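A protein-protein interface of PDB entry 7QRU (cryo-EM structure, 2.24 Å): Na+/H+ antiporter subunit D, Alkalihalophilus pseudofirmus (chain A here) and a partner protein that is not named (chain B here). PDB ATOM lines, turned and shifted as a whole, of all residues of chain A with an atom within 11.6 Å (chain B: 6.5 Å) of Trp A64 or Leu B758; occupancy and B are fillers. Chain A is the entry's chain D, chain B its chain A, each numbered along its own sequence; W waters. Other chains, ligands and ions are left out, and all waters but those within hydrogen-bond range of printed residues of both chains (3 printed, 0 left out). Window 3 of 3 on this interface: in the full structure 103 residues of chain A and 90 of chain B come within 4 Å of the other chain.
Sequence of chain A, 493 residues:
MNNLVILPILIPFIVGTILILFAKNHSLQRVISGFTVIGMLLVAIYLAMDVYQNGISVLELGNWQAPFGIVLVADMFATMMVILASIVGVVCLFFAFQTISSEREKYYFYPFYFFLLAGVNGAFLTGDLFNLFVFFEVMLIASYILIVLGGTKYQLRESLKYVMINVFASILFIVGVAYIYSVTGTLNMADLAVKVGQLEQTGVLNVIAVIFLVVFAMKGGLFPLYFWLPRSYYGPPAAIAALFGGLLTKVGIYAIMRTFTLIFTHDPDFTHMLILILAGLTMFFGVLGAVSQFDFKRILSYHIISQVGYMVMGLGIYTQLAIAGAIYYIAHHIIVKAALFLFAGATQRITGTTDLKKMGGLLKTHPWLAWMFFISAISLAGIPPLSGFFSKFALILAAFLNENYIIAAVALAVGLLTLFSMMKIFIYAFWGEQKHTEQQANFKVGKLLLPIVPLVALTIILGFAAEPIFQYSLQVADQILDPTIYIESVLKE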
ATOM      1  N   MET A   1     -26.724 -21.699  -8.059  1.00  0.00           N
ATOM      2  CA  MET A   1     -25.419 -21.659  -7.345  1.00  0.00           C
ATOM      3  C   MET A   1     -25.502 -20.598  -6.247  1.00  0.00           C
ATOM      4  O   MET A   1     -25.707 -20.958  -5.107  1.00  0.00           O
ATOM      5  CB  MET A   1     -24.276 -21.339  -8.316  1.00  0.00           C
ATOM      6  CG  MET A   1     -22.891 -21.305  -7.677  1.00  0.00           C
ATOM      7  SD  MET A   1     -21.762 -20.007  -8.337  1.00  0.00           S
ATOM      8  CE  MET A   1     -21.727 -20.371 -10.094  1.00  0.00           C
ATOM      9  N   ASN A   2     -25.349 -19.313  -6.592  1.00  0.00           N
ATOM     10  CA  ASN A   2     -25.329 -18.203  -5.669  1.00  0.00           C
ATOM     11  C   ASN A   2     -24.204 -18.308  -4.633  1.00  0.00           C
ATOM     12  O   ASN A   2     -24.448 -18.024  -3.459  1.00  0.00           O
ATOM     13  CB  ASN A   2     -26.718 -18.049  -5.036  1.00  0.00           C
ATOM     14  CG  ASN A   2     -27.811 -17.761  -6.052  1.00  0.00           C
ATOM     15  OD1 ASN A   2     -27.541 -17.211  -7.123  1.00  0.00           O
ATOM     16  ND2 ASN A   2     -29.042 -18.128  -5.727  1.00  0.00           N
ATOM     17  N   ASN A   3     -23.034 -18.861  -4.980  1.00  0.00           N
ATOM     18  CA  ASN A   3     -21.923 -18.960  -4.069  1.00  0.00           C
ATOM     19  C   ASN A   3     -21.356 -17.585  -3.672  1.00  0.00           C
ATOM     20  O   ASN A   3     -20.721 -17.439  -2.625  1.00  0.00           O
ATOM     21  CB  ASN A   3     -20.834 -19.886  -4.589  1.00  0.00           C
ATOM     22  CG  ASN A   3     -21.008 -21.359  -4.284  1.00  0.00           C
ATOM     23  OD1 ASN A   3     -21.351 -21.714  -3.172  1.00  0.00           O
ATOM     24  ND2 ASN A   3     -20.701 -22.240  -5.216  1.00  0.00           N
ATOM     25  N   VAL A  58     -30.756 -17.016  -2.878  1.00  0.00           N
ATOM     26  CA  VAL A  58     -30.724 -18.054  -1.869  1.00  0.00           C
ATOM     27  C   VAL A  58     -29.594 -19.028  -2.174  1.00  0.00           C
ATOM     28  O   VAL A  58     -29.541 -19.470  -3.266  1.00  0.00           O
ATOM     29  CB  VAL A  58     -32.100 -18.752  -1.779  1.00  0.00           C
ATOM     30  CG1 VAL A  58     -32.107 -19.860  -0.763  1.00  0.00           C
ATOM     31  CG2 VAL A  58     -33.119 -17.694  -1.409  1.00  0.00           C
ATOM     32  N   LEU A  59     -28.719 -19.343  -1.244  1.00  0.00           N
ATOM     33  CA  LEU A  59     -27.684 -20.360  -1.383  1.00  0.00           C
ATOM     34  C   LEU A  59     -28.010 -21.544  -0.476  1.00  0.00           C
ATOM     35  O   LEU A  59     -28.156 -21.371   0.739  1.00  0.00           O
ATOM     36  CB  LEU A  59     -26.356 -19.759  -0.965  1.00  0.00           C
ATOM     37  CG  LEU A  59     -25.154 -20.702  -0.884  1.00  0.00           C
ATOM     38  CD1 LEU A  59     -24.884 -21.338  -2.210  1.00  0.00           C
ATOM     39  CD2 LEU A  59     -23.915 -19.993  -0.399  1.00  0.00           C
ATOM     40  N   GLU A  60     -28.174 -22.737  -1.032  1.00  0.00           N
ATOM     41  CA  GLU A  60     -28.415 -23.935  -0.234  1.00  0.00           C
ATOM     42  C   GLU A  60     -27.138 -24.689   0.073  1.00  0.00           C
ATOM     43  O   GLU A  60     -26.710 -25.467  -0.735  1.00  0.00           O
ATOM     44  CB  GLU A  60     -29.397 -24.818  -0.975  1.00  0.00           C
ATOM     45  CG  GLU A  60     -30.605 -24.088  -1.301  1.00  0.00           C
ATOM     46  CD  GLU A  60     -31.612 -24.838  -2.128  1.00  0.00           C
ATOM     47  OE1 GLU A  60     -31.255 -25.920  -2.690  1.00  0.00           O
ATOM     48  OE2 GLU A  60     -32.793 -24.357  -2.152  1.00  0.00           O
ATOM     49  N   LEU A  61     -26.582 -24.503   1.243  1.00  0.00           N
ATOM     50  CA  LEU A  61     -25.306 -25.100   1.612  1.00  0.00           C
ATOM     51  C   LEU A  61     -25.405 -26.637   1.602  1.00  0.00           C
ATOM     52  O   LEU A  61     -26.381 -27.204   2.081  1.00  0.00           O
ATOM     53  CB  LEU A  61     -24.979 -24.593   2.994  1.00  0.00           C
ATOM     54  CG  LEU A  61     -24.616 -23.107   3.028  1.00  0.00           C
ATOM     55  CD1 LEU A  61     -24.287 -22.726   4.403  1.00  0.00           C
ATOM     56  CD2 LEU A  61     -23.414 -22.832   2.196  1.00  0.00           C
ATOM     57  N   GLY A  62     -24.469 -27.294   0.905  1.00  0.00           N
ATOM     58  CA  GLY A  62     -24.419 -28.741   0.835  1.00  0.00           C
ATOM     59  C   GLY A  62     -25.322 -29.290  -0.242  1.00  0.00           C
ATOM     60  O   GLY A  62     -25.385 -30.531  -0.439  1.00  0.00           O
ATOM     61  N   ASN A  63     -25.866 -28.339  -0.956  1.00  0.00           N
ATOM     62  CA  ASN A  63     -26.865 -28.546  -1.993  1.00  0.00           C
ATOM     63  C   ASN A  63     -28.176 -29.119  -1.466  1.00  0.00           C
ATOM     64  O   ASN A  63     -28.848 -29.825  -2.176  1.00  0.00           O
ATOM     65  CB  ASN A  63     -26.203 -29.435  -3.048  1.00  0.00           C
ATOM     66  CG  ASN A  63     -26.677 -29.126  -4.444  1.00  0.00           C
ATOM     67  OD1 ASN A  63     -27.299 -28.099  -4.689  1.00  0.00           O
ATOM     68  ND2 ASN A  63     -26.247 -29.933  -5.379  1.00  0.00           N
ATOM     69  N   TRP A  64     -28.442 -29.042  -0.162  1.00  0.00           N
ATOM     70  CA  TRP A  64     -29.695 -29.552   0.340  1.00  0.00           C
ATOM     71  C   TRP A  64     -30.727 -28.437   0.305  1.00  0.00           C
ATOM     72  O   TRP A  64     -30.424 -27.351   0.800  1.00  0.00           O
ATOM     73  CB  TRP A  64     -29.521 -29.991   1.760  1.00  0.00           C
ATOM     74  CG  TRP A  64     -28.391 -30.938   1.913  1.00  0.00           C
ATOM     75  CD1 TRP A  64     -27.196 -30.762   2.546  1.00  0.00           C
ATOM     76  CD2 TRP A  64     -28.435 -32.265   1.450  1.00  0.00           C
ATOM     77  NE1 TRP A  64     -26.462 -31.920   2.473  1.00  0.00           N
ATOM     78  CE2 TRP A  64     -27.205 -32.852   1.815  1.00  0.00           C
ATOM     79  CE3 TRP A  64     -29.398 -32.979   0.747  1.00  0.00           C
ATOM     80  CZ2 TRP A  64     -26.908 -34.172   1.446  1.00  0.00           C
ATOM     81  CZ3 TRP A  64     -29.140 -34.305   0.414  1.00  0.00           C
ATOM     82  CH2 TRP A  64     -27.922 -34.882   0.773  1.00  0.00           C
ATOM     83  N   GLN A  65     -31.918 -28.713  -0.243  1.00  0.00           N
ATOM     84  CA  GLN A  65     -32.967 -27.681  -0.307  1.00  0.00           C
ATOM     85  C   GLN A  65     -33.463 -27.334   1.090  1.00  0.00           C
ATOM     86  O   GLN A  65     -33.456 -28.169   1.954  1.00  0.00           O
ATOM     87  CB  GLN A  65     -34.123 -28.148  -1.193  1.00  0.00           C
ATOM     88  CG  GLN A  65     -34.846 -29.391  -0.693  1.00  0.00           C
ATOM     89  CD  GLN A  65     -34.243 -30.749  -0.957  1.00  0.00           C
ATOM     90  OE1 GLN A  65     -33.120 -30.929  -1.455  1.00  0.00           O
ATOM     91  NE2 GLN A  65     -35.060 -31.759  -0.667  1.00  0.00           N
ATOM     92  N   ALA A  66     -33.940 -26.121   1.342  1.00  0.00           N
ATOM     93  CA  ALA A  66     -34.635 -25.775   2.567  1.00  0.00           C
ATOM     94  C   ALA A  66     -35.945 -26.571   2.604  1.00  0.00           C
ATOM     95  O   ALA A  66     -36.614 -26.778   1.599  1.00  0.00           O
ATOM     96  CB  ALA A  66     -34.904 -24.299   2.639  1.00  0.00           C
ATOM     97  N   PRO A  67     -36.428 -26.998   3.783  1.00  0.00           N
ATOM     98  CA  PRO A  67     -35.847 -26.696   5.072  1.00  0.00           C
ATOM     99  C   PRO A  67     -34.845 -27.687   5.649  1.00  0.00           C
ATOM    100  O   PRO A  67     -34.354 -27.497   6.737  1.00  0.00           O
ATOM    101  CB  PRO A  67     -37.112 -26.712   5.905  1.00  0.00           C
ATOM    102  CG  PRO A  67     -37.798 -27.877   5.405  1.00  0.00           C
ATOM    103  CD  PRO A  67     -37.563 -27.864   3.918  1.00  0.00           C
ATOM    104  N   PHE A  68     -34.398 -28.640   4.865  1.00  0.00           N
ATOM    105  CA  PHE A  68     -33.486 -29.684   5.335  1.00  0.00           C
ATOM    106  C   PHE A  68     -32.080 -29.172   5.560  1.00  0.00           C
ATOM    107  O   PHE A  68     -31.413 -29.551   6.507  1.00  0.00           O
ATOM    108  CB  PHE A  68     -33.480 -30.847   4.344  1.00  0.00           C
ATOM    109  CG  PHE A  68     -34.860 -31.278   4.025  1.00  0.00           C
ATOM    110  CD1 PHE A  68     -35.740 -31.641   5.039  1.00  0.00           C
ATOM    111  CD2 PHE A  68     -35.306 -31.130   2.760  1.00  0.00           C
ATOM    112  CE1 PHE A  68     -37.091 -31.800   4.746  1.00  0.00           C
ATOM    113  CE2 PHE A  68     -36.623 -31.434   2.473  1.00  0.00           C
ATOM    114  CZ  PHE A  68     -37.502 -31.798   3.442  1.00  0.00           C
ATOM    115  N   GLY A  69     -31.617 -28.323   4.700  1.00  0.00           N
ATOM    116  CA  GLY A  69     -30.256 -27.804   4.810  1.00  0.00           C
ATOM    117  C   GLY A  69     -30.279 -26.347   5.355  1.00  0.00           C
ATOM    118  O   GLY A  69     -31.306 -25.614   5.345  1.00  0.00           O
ATOM    119  N   ILE A  70     -29.124 -25.896   5.786  1.00  0.00           N
ATOM    120  CA  ILE A  70     -28.940 -24.492   6.114  1.00  0.00           C
ATOM    121  C   ILE A  70     -29.050 -23.681   4.816  1.00  0.00           C
ATOM    122  O   ILE A  70     -28.425 -24.065   3.879  1.00  0.00           O
ATOM    123  CB  ILE A  70     -27.605 -24.336   6.830  1.00  0.00           C
ATOM    124  CG1 ILE A  70     -27.700 -25.060   8.183  1.00  0.00           C
ATOM    125  CG2 ILE A  70     -27.253 -22.852   6.911  1.00  0.00           C
ATOM    126  CD1 ILE A  70     -26.370 -25.308   8.868  1.00  0.00           C
ATOM    127  N   VAL A  71     -29.973 -22.714   4.664  1.00  0.00           N
ATOM    128  CA  VAL A  71     -29.890 -21.754   3.550  1.00  0.00           C
ATOM    129  C   VAL A  71     -29.281 -20.433   3.996  1.00  0.00           C
ATOM    130  O   VAL A  71     -29.571 -20.036   5.097  1.00  0.00           O
ATOM    131  CB  VAL A  71     -31.251 -21.543   2.869  1.00  0.00           C
ATOM    132  CG1 VAL A  71     -31.609 -22.851   2.222  1.00  0.00           C
ATOM    133  CG2 VAL A  71     -32.273 -21.155   3.902  1.00  0.00           C
ATOM    134  N   LEU A  72     -28.520 -19.737   3.139  1.00  0.00           N
ATOM    135  CA  LEU A  72     -28.282 -18.308   3.297  1.00  0.00           C
ATOM    136  C   LEU A  72     -29.154 -17.558   2.302  1.00  0.00           C
ATOM    137  O   LEU A  72     -29.434 -18.062   1.162  1.00  0.00           O
ATOM    138  CB  LEU A  72     -26.843 -17.963   3.012  1.00  0.00           C
ATOM    139  CG  LEU A  72     -25.796 -18.763   3.763  1.00  0.00           C
ATOM    140  CD1 LEU A  72     -24.403 -18.333   3.338  1.00  0.00           C
ATOM    141  CD2 LEU A  72     -25.952 -18.618   5.247  1.00  0.00           C
ATOM    142  N   VAL A  73     -29.720 -16.455   2.794  1.00  0.00           N
ATOM    143  CA  VAL A  73     -30.717 -15.720   2.013  1.00  0.00           C
ATOM    144  C   VAL A  73     -30.221 -14.298   1.893  1.00  0.00           C
ATOM    145  O   VAL A  73     -30.253 -13.594   2.852  1.00  0.00           O
ATOM    146  CB  VAL A  73     -32.115 -15.718   2.678  1.00  0.00           C
ATOM    147  CG1 VAL A  73     -33.159 -15.105   1.765  1.00  0.00           C
ATOM    148  CG2 VAL A  73     -32.578 -17.118   3.059  1.00  0.00           C
ATOM    149  N   GLY A 127     -30.812 -17.954   6.798  1.00  0.00           N
ATOM    150  CA  GLY A 127     -32.230 -18.292   6.799  1.00  0.00           C
ATOM    151  C   GLY A 127     -32.593 -19.394   7.760  1.00  0.00           C
ATOM    152  O   GLY A 127     -33.618 -19.992   7.559  1.00  0.00           O
ATOM    153  N   ASP A 128     -31.783 -19.649   8.785  1.00  0.00           N
ATOM    154  CA  ASP A 128     -32.025 -20.775   9.686  1.00  0.00           C
ATOM    155  C   ASP A 128     -31.853 -20.297  11.127  1.00  0.00           C
ATOM    156  O   ASP A 128     -30.764 -19.871  11.489  1.00  0.00           O
ATOM    157  CB  ASP A 128     -31.014 -21.907   9.368  1.00  0.00           C
ATOM    158  CG  ASP A 128     -31.237 -23.217  10.150  1.00  0.00           C
ATOM    159  OD1 ASP A 128     -30.893 -23.276  11.318  1.00  0.00           O
ATOM    160  OD2 ASP A 128     -31.835 -24.209   9.594  1.00  0.00           O
ATOM    161  N   ASN A 188     -35.876 -23.799   9.890  1.00  0.00           N
ATOM    162  CA  ASN A 188     -35.759 -22.927   8.751  1.00  0.00           C
ATOM    163  C   ASN A 188     -36.730 -21.762   8.942  1.00  0.00           C
ATOM    164  O   ASN A 188     -37.909 -22.009   9.225  1.00  0.00           O
ATOM    165  CB  ASN A 188     -36.089 -23.647   7.449  1.00  0.00           C
ATOM    166  CG  ASN A 188     -35.996 -22.760   6.216  1.00  0.00           C
ATOM    167  OD1 ASN A 188     -36.954 -22.600   5.469  1.00  0.00           O
ATOM    168  ND2 ASN A 188     -34.862 -22.176   5.933  1.00  0.00           N
ATOM    169  N   SER A 489     -38.959 -17.406  -2.209  1.00  0.00           N
ATOM    170  CA  SER A 489     -37.549 -17.474  -2.511  1.00  0.00           C
ATOM    171  C   SER A 489     -36.945 -18.747  -1.957  1.00  0.00           C
ATOM    172  O   SER A 489     -36.104 -19.286  -2.592  1.00  0.00           O
ATOM    173  CB  SER A 489     -36.834 -16.265  -1.981  1.00  0.00           C
ATOM    174  OG  SER A 489     -37.412 -15.157  -2.670  1.00  0.00           O
ATOM    175  N   VAL A 490     -37.314 -19.167  -0.779  1.00  0.00           N
ATOM    176  CA  VAL A 490     -36.612 -20.199  -0.071  1.00  0.00           C
ATOM    177  C   VAL A 490     -37.372 -21.513  -0.246  1.00  0.00           C
ATOM    178  O   VAL A 490     -36.767 -22.512  -0.259  1.00  0.00           O
ATOM    179  CB  VAL A 490     -36.469 -19.793   1.401  1.00  0.00           C
ATOM    180  CG1 VAL A 490     -35.958 -20.935   2.270  1.00  0.00           C
ATOM    181  CG2 VAL A 490     -35.609 -18.577   1.531  1.00  0.00           C
ATOM    182  N   LEU A 491     -38.683 -21.559  -0.295  1.00  0.00           N
ATOM    183  CA  LEU A 491     -39.371 -22.843  -0.339  1.00  0.00           C
ATOM    184  C   LEU A 491     -40.126 -23.053  -1.661  1.00  0.00           C
ATOM    185  O   LEU A 491     -39.457 -22.993  -2.760  1.00  0.00           O
ATOM    186  CB  LEU A 491     -40.419 -22.820   0.767  1.00  0.00           C
ATOM    187  CG  LEU A 491     -39.889 -22.806   2.185  1.00  0.00           C
ATOM    188  CD1 LEU A 491     -41.087 -22.747   3.101  1.00  0.00           C
ATOM    189  CD2 LEU A 491     -39.033 -24.011   2.443  1.00  0.00           C
ATOM    190  N   PHE B 750     -36.648 -36.557   6.767  1.00  0.00           N
ATOM    191  CA  PHE B 750     -35.852 -36.587   5.545  1.00  0.00           C
ATOM    192  C   PHE B 750     -34.462 -37.205   5.758  1.00  0.00           C
ATOM    193  O   PHE B 750     -33.904 -37.849   4.880  1.00  0.00           O
ATOM    194  CB  PHE B 750     -35.794 -35.138   5.053  1.00  0.00           C
ATOM    195  CG  PHE B 750     -34.915 -34.937   3.871  1.00  0.00           C
ATOM    196  CD1 PHE B 750     -35.451 -34.935   2.622  1.00  0.00           C
ATOM    197  CD2 PHE B 750     -33.587 -34.602   4.039  1.00  0.00           C
ATOM    198  CE1 PHE B 750     -34.657 -34.702   1.515  1.00  0.00           C
ATOM    199  CE2 PHE B 750     -32.777 -34.359   2.946  1.00  0.00           C
ATOM    200  CZ  PHE B 750     -33.310 -34.437   1.670  1.00  0.00           C
ATOM    201  N   GLU B 753     -34.772 -40.853   5.892  1.00  0.00           N
ATOM    202  CA  GLU B 753     -34.893 -41.486   4.583  1.00  0.00           C
ATOM    203  C   GLU B 753     -33.582 -41.512   3.795  1.00  0.00           C
ATOM    204  O   GLU B 753     -33.332 -42.457   3.064  1.00  0.00           O
ATOM    205  CB  GLU B 753     -35.965 -40.791   3.755  1.00  0.00           C
ATOM    206  CG  GLU B 753     -37.369 -41.058   4.279  1.00  0.00           C
ATOM    207  CD  GLU B 753     -38.399 -40.014   3.850  1.00  0.00           C
ATOM    208  OE1 GLU B 753     -39.562 -40.022   4.400  1.00  0.00           O
ATOM    209  OE2 GLU B 753     -38.037 -39.176   2.961  1.00  0.00           O
ATOM    210  N   ASN B 754     -32.799 -40.462   3.884  1.00  0.00           N
ATOM    211  CA  ASN B 754     -31.769 -40.126   2.924  1.00  0.00           C
ATOM    212  C   ASN B 754     -30.397 -40.084   3.549  1.00  0.00           C
ATOM    213  O   ASN B 754     -29.453 -39.931   2.791  1.00  0.00           O
ATOM    214  CB  ASN B 754     -32.057 -38.739   2.359  1.00  0.00           C
ATOM    215  CG  ASN B 754     -33.355 -38.813   1.578  1.00  0.00           C
ATOM    216  OD1 ASN B 754     -33.459 -39.587   0.629  1.00  0.00           O
ATOM    217  ND2 ASN B 754     -34.361 -38.073   1.980  1.00  0.00           N
ATOM    218  N   SER B 755     -30.222 -40.328   4.864  1.00  0.00           N
ATOM    219  CA  SER B 755     -28.848 -40.323   5.357  1.00  0.00           C
ATOM    220  C   SER B 755     -28.022 -41.364   4.630  1.00  0.00           C
ATOM    221  O   SER B 755     -26.835 -41.133   4.464  1.00  0.00           O
ATOM    222  CB  SER B 755     -28.641 -40.547   6.841  1.00  0.00           C
ATOM    223  OG  SER B 755     -29.207 -39.463   7.490  1.00  0.00           O
ATOM    224  N   LYS B 756     -28.518 -42.578   4.377  1.00  0.00           N
ATOM    225  CA  LYS B 756     -27.545 -43.515   3.833  1.00  0.00           C
ATOM    226  C   LYS B 756     -27.510 -43.345   2.310  1.00  0.00           C
ATOM    227  O   LYS B 756     -26.423 -43.212   1.785  1.00  0.00           O
ATOM    228  CB  LYS B 756     -27.783 -44.975   4.224  1.00  0.00           C
ATOM    229  CG  LYS B 756     -26.768 -45.963   3.641  1.00  0.00           C
ATOM    230  CD  LYS B 756     -25.370 -45.675   4.194  1.00  0.00           C
ATOM    231  CE  LYS B 756     -24.362 -46.805   4.097  1.00  0.00           C
ATOM    232  NZ  LYS B 756     -24.467 -47.401   2.749  1.00  0.00           N
ATOM    233  N   GLU B 757     -28.650 -43.220   1.649  1.00  0.00           N
ATOM    234  CA  GLU B 757     -28.697 -43.111   0.197  1.00  0.00           C
ATOM    235  C   GLU B 757     -28.041 -41.830  -0.325  1.00  0.00           C
ATOM    236  O   GLU B 757     -27.152 -41.934  -1.163  1.00  0.00           O
ATOM    237  CB  GLU B 757     -30.106 -43.306  -0.366  1.00  0.00           C
ATOM    238  CG  GLU B 757     -31.188 -42.443   0.233  1.00  0.00           C
ATOM    239  CD  GLU B 757     -32.488 -42.333  -0.575  1.00  0.00           C
ATOM    240  OE1 GLU B 757     -32.403 -42.215  -1.830  1.00  0.00           O
ATOM    241  OE2 GLU B 757     -33.605 -42.342   0.044  1.00  0.00           O
ATOM    242  N   LEU B 758     -28.344 -40.660   0.218  1.00  0.00           N
ATOM    243  CA  LEU B 758     -27.791 -39.426  -0.331  1.00  0.00           C
ATOM    244  C   LEU B 758     -26.602 -38.960   0.436  1.00  0.00           C
ATOM    245  O   LEU B 758     -25.978 -38.019   0.008  1.00  0.00           O
ATOM    246  CB  LEU B 758     -28.841 -38.313  -0.308  1.00  0.00           C
ATOM    247  CG  LEU B 758     -30.137 -38.704  -1.009  1.00  0.00           C
ATOM    248  CD1 LEU B 758     -31.063 -37.554  -0.997  1.00  0.00           C
ATOM    249  CD2 LEU B 758     -29.836 -39.065  -2.408  1.00  0.00           C
ATOM    250  N   ALA B 759     -26.219 -39.545   1.540  1.00  0.00           N
ATOM    251  CA  ALA B 759     -25.059 -38.952   2.198  1.00  0.00           C
ATOM    252  C   ALA B 759     -24.135 -40.020   2.679  1.00  0.00           C
ATOM    253  O   ALA B 759     -23.142 -39.708   3.290  1.00  0.00           O
ATOM    254  CB  ALA B 759     -25.496 -38.035   3.306  1.00  0.00           C
ATOM    255  N   GLY B 760     -24.433 -41.264   2.343  1.00  0.00           N
ATOM    256  CA  GLY B 760     -23.499 -42.302   2.626  1.00  0.00           C
ATOM    257  C   GLY B 760     -23.190 -42.645   4.087  1.00  0.00           C
ATOM    258  O   GLY B 760     -22.264 -43.392   4.287  1.00  0.00           O
ATOM    259  N   GLY B 761     -23.981 -42.297   5.104  1.00  0.00           N
ATOM    260  CA  GLY B 761     -23.637 -42.799   6.423  1.00  0.00           C
ATOM    261  C   GLY B 761     -24.832 -43.414   7.107  1.00  0.00           C
ATOM    262  O   GLY B 761     -25.928 -43.067   6.784  1.00  0.00           O
ATOM    263  N   ASP B 771     -22.857 -33.107   6.939  1.00  0.00           N
ATOM    264  CA  ASP B 771     -23.395 -33.045   5.606  1.00  0.00           C
ATOM    265  C   ASP B 771     -24.654 -32.171   5.508  1.00  0.00           C
ATOM    266  O   ASP B 771     -24.598 -31.122   4.875  1.00  0.00           O
ATOM    267  CB  ASP B 771     -23.552 -34.425   5.016  1.00  0.00           C
ATOM    268  CG  ASP B 771     -23.762 -34.355   3.530  1.00  0.00           C
ATOM    269  OD1 ASP B 771     -24.204 -33.264   3.052  1.00  0.00           O
ATOM    270  OD2 ASP B 771     -23.433 -35.365   2.839  1.00  0.00           O
ATOM    271  N   PHE B 772     -25.766 -32.510   6.134  1.00  0.00           N
ATOM    272  CA  PHE B 772     -26.966 -31.706   5.940  1.00  0.00           C
ATOM    273  C   PHE B 772     -26.872 -30.363   6.592  1.00  0.00           C
ATOM    274  O   PHE B 772     -27.400 -29.467   5.992  1.00  0.00           O
ATOM    275  CB  PHE B 772     -28.185 -32.400   6.476  1.00  0.00           C
ATOM    276  CG  PHE B 772     -28.438 -33.710   5.769  1.00  0.00           C
ATOM    277  CD1 PHE B 772     -29.055 -33.703   4.550  1.00  0.00           C
ATOM    278  CD2 PHE B 772     -28.319 -34.932   6.442  1.00  0.00           C
ATOM    279  CE1 PHE B 772     -29.417 -34.904   3.948  1.00  0.00           C
ATOM    280  CE2 PHE B 772     -28.726 -36.134   5.859  1.00  0.00           C
ATOM    281  CZ  PHE B 772     -29.186 -36.102   4.570  1.00  0.00           C
ATOM    282  N   ARG B 773     -26.007 -30.197   7.606  1.00  0.00           N
ATOM    283  CA  ARG B 773     -25.942 -28.993   8.392  1.00  0.00           C
ATOM    284  C   ARG B 773     -24.509 -28.729   8.761  1.00  0.00           C
ATOM    285  O   ARG B 773     -24.205 -28.318   9.895  1.00  0.00           O
ATOM    286  CB  ARG B 773     -26.810 -28.994   9.694  1.00  0.00           C
ATOM    287  CG  ARG B 773     -28.309 -29.107   9.351  1.00  0.00           C
ATOM    288  CD  ARG B 773     -29.178 -28.959  10.574  1.00  0.00           C
ATOM    289  NE  ARG B 773     -28.826 -27.808  11.388  1.00  0.00           N
ATOM    290  CZ  ARG B 773     -29.523 -26.670  11.215  1.00  0.00           C
ATOM    291  NH1 ARG B 773     -30.623 -26.670  10.452  1.00  0.00           N
ATOM    292  NH2 ARG B 773     -29.044 -25.538  11.694  1.00  0.00           N
HETATM  293  O   HOH W   1     -26.632 -27.457   4.798  1.00  0.00           O
HETATM  294  O   HOH W   2     -31.878 -28.476   8.922  1.00  0.00           O
HETATM  295  O   HOH W   3     -23.431 -32.352   0.766  1.00  0.00           O
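The guanidinium group of Arg B773 lies within salt-bridge range of the side-chain carboxylate of Asp A128.
The indole nitrogen (NE1) of Trp A64 lies within hydrogen-bond range of the side-chain carboxylate (OD1) of Asp B771, at 2.7 Å.
The backbone carbonyl oxygen (O) of Gly A62 lies within hydrogen-bond range of the indole nitrogen (NE1) of Trp A64, at 3.4 Å.
O of Ile A70 sits at hydrogen-bond distance from N of Leu A61 (3.2 Å).
The backbone carbonyl oxygen (O) of Phe B750 sits at hydrogen-bond distance from the side-chain amide nitrogen (ND2) of Asn B754 (2.9 Å).
Among the printed residues, merely in contact across the chains: Trp A64 with Phe B772 (3.4 Å), Phe A68 with Phe B750 (3.5 Å), Gly A69 with Phe B772 (3.5 Å), Gln A65 with Phe B750 (3.7 Å), Trp A64 with Leu B758 (3.7 Å), Ile A70 with Arg B773 (3.7 Å) and Ile A70 with Phe B772 (3.97 Å).
Of chain B, only Leu B758 (3.7 Å), Asp B771 (2.7 Å) and Phe B772 (3.4 Å) come within 4 Å of Trp A64.
Of the printed residues of chain B, Phe A68 touches Phe B750.
Of the printed residues of chain B, Gly A69 touches Phe B772 (3.5 Å).
Printed residues of chain B within 4 Å of Asp A128: Arg B773.
No residue of chain A comes within 4 Å of Asn B754.
No residue of chain A comes within 4 Å of Ser B755.
No residue of chain A comes within 4 Å of Glu B757.
Of chain A, only Trp A64 (3.7 Å) comes within 4 Å of Leu B758.
Of chain A, only Trp A64 comes within 4 Å of Asp B771.
Of chain A, only Trp A64 (3.4 Å), Gly A69 (3.5 Å) and Ile A70 (3.97 Å) come within 4 Å of Phe B772.
Of the printed residues of chain A, Arg B773 touches Ile A70 (3.7 Å) and Asp A128 (2.9 Å).
The nearest residue of chain A that does not touch Leu B758 is Gln A65 (7.0 Å).
The nearest printed residue of chain B that does not touch Gln A65 is Asn B754 (6.9 Å).
Printed residues of chain A that touch a printed residue of chain B: Trp A64, Gln A65, Phe A68, Gly A69, Ile A70 and Asp A128.
Hydrophobic or aromatic side chains of chain A that line the printed part of chain B: Trp A64, Phe A68 and Ile A70.
Among the printed residues, Asp or Glu carboxylates within 4 Å of a Lys or Arg side-chain nitrogen of the other chain: Asp A128 with Arg B773 (2.9 Å).
Water W1 lies within hydrogen-bond range of the backbone carbonyl oxygen (O) of Phe B772, the backbone carbonyl oxygen (O) of Leu A61 and the backbone NH (N) of Ile A70.
Water W3 bridges the side-chain carboxylate of Asp B771 (2.6 Å) and the backbone carbonyl oxygen of Gly A62 (2.9 Å).
Water W2 lies within hydrogen-bond range of the guanidinium group of Arg B773 (2.7 Å), the backbone carbonyl oxygen of Phe A68 (2.7 Å) and the backbone carbonyl oxygen of Pro A67 (3.4 Å).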
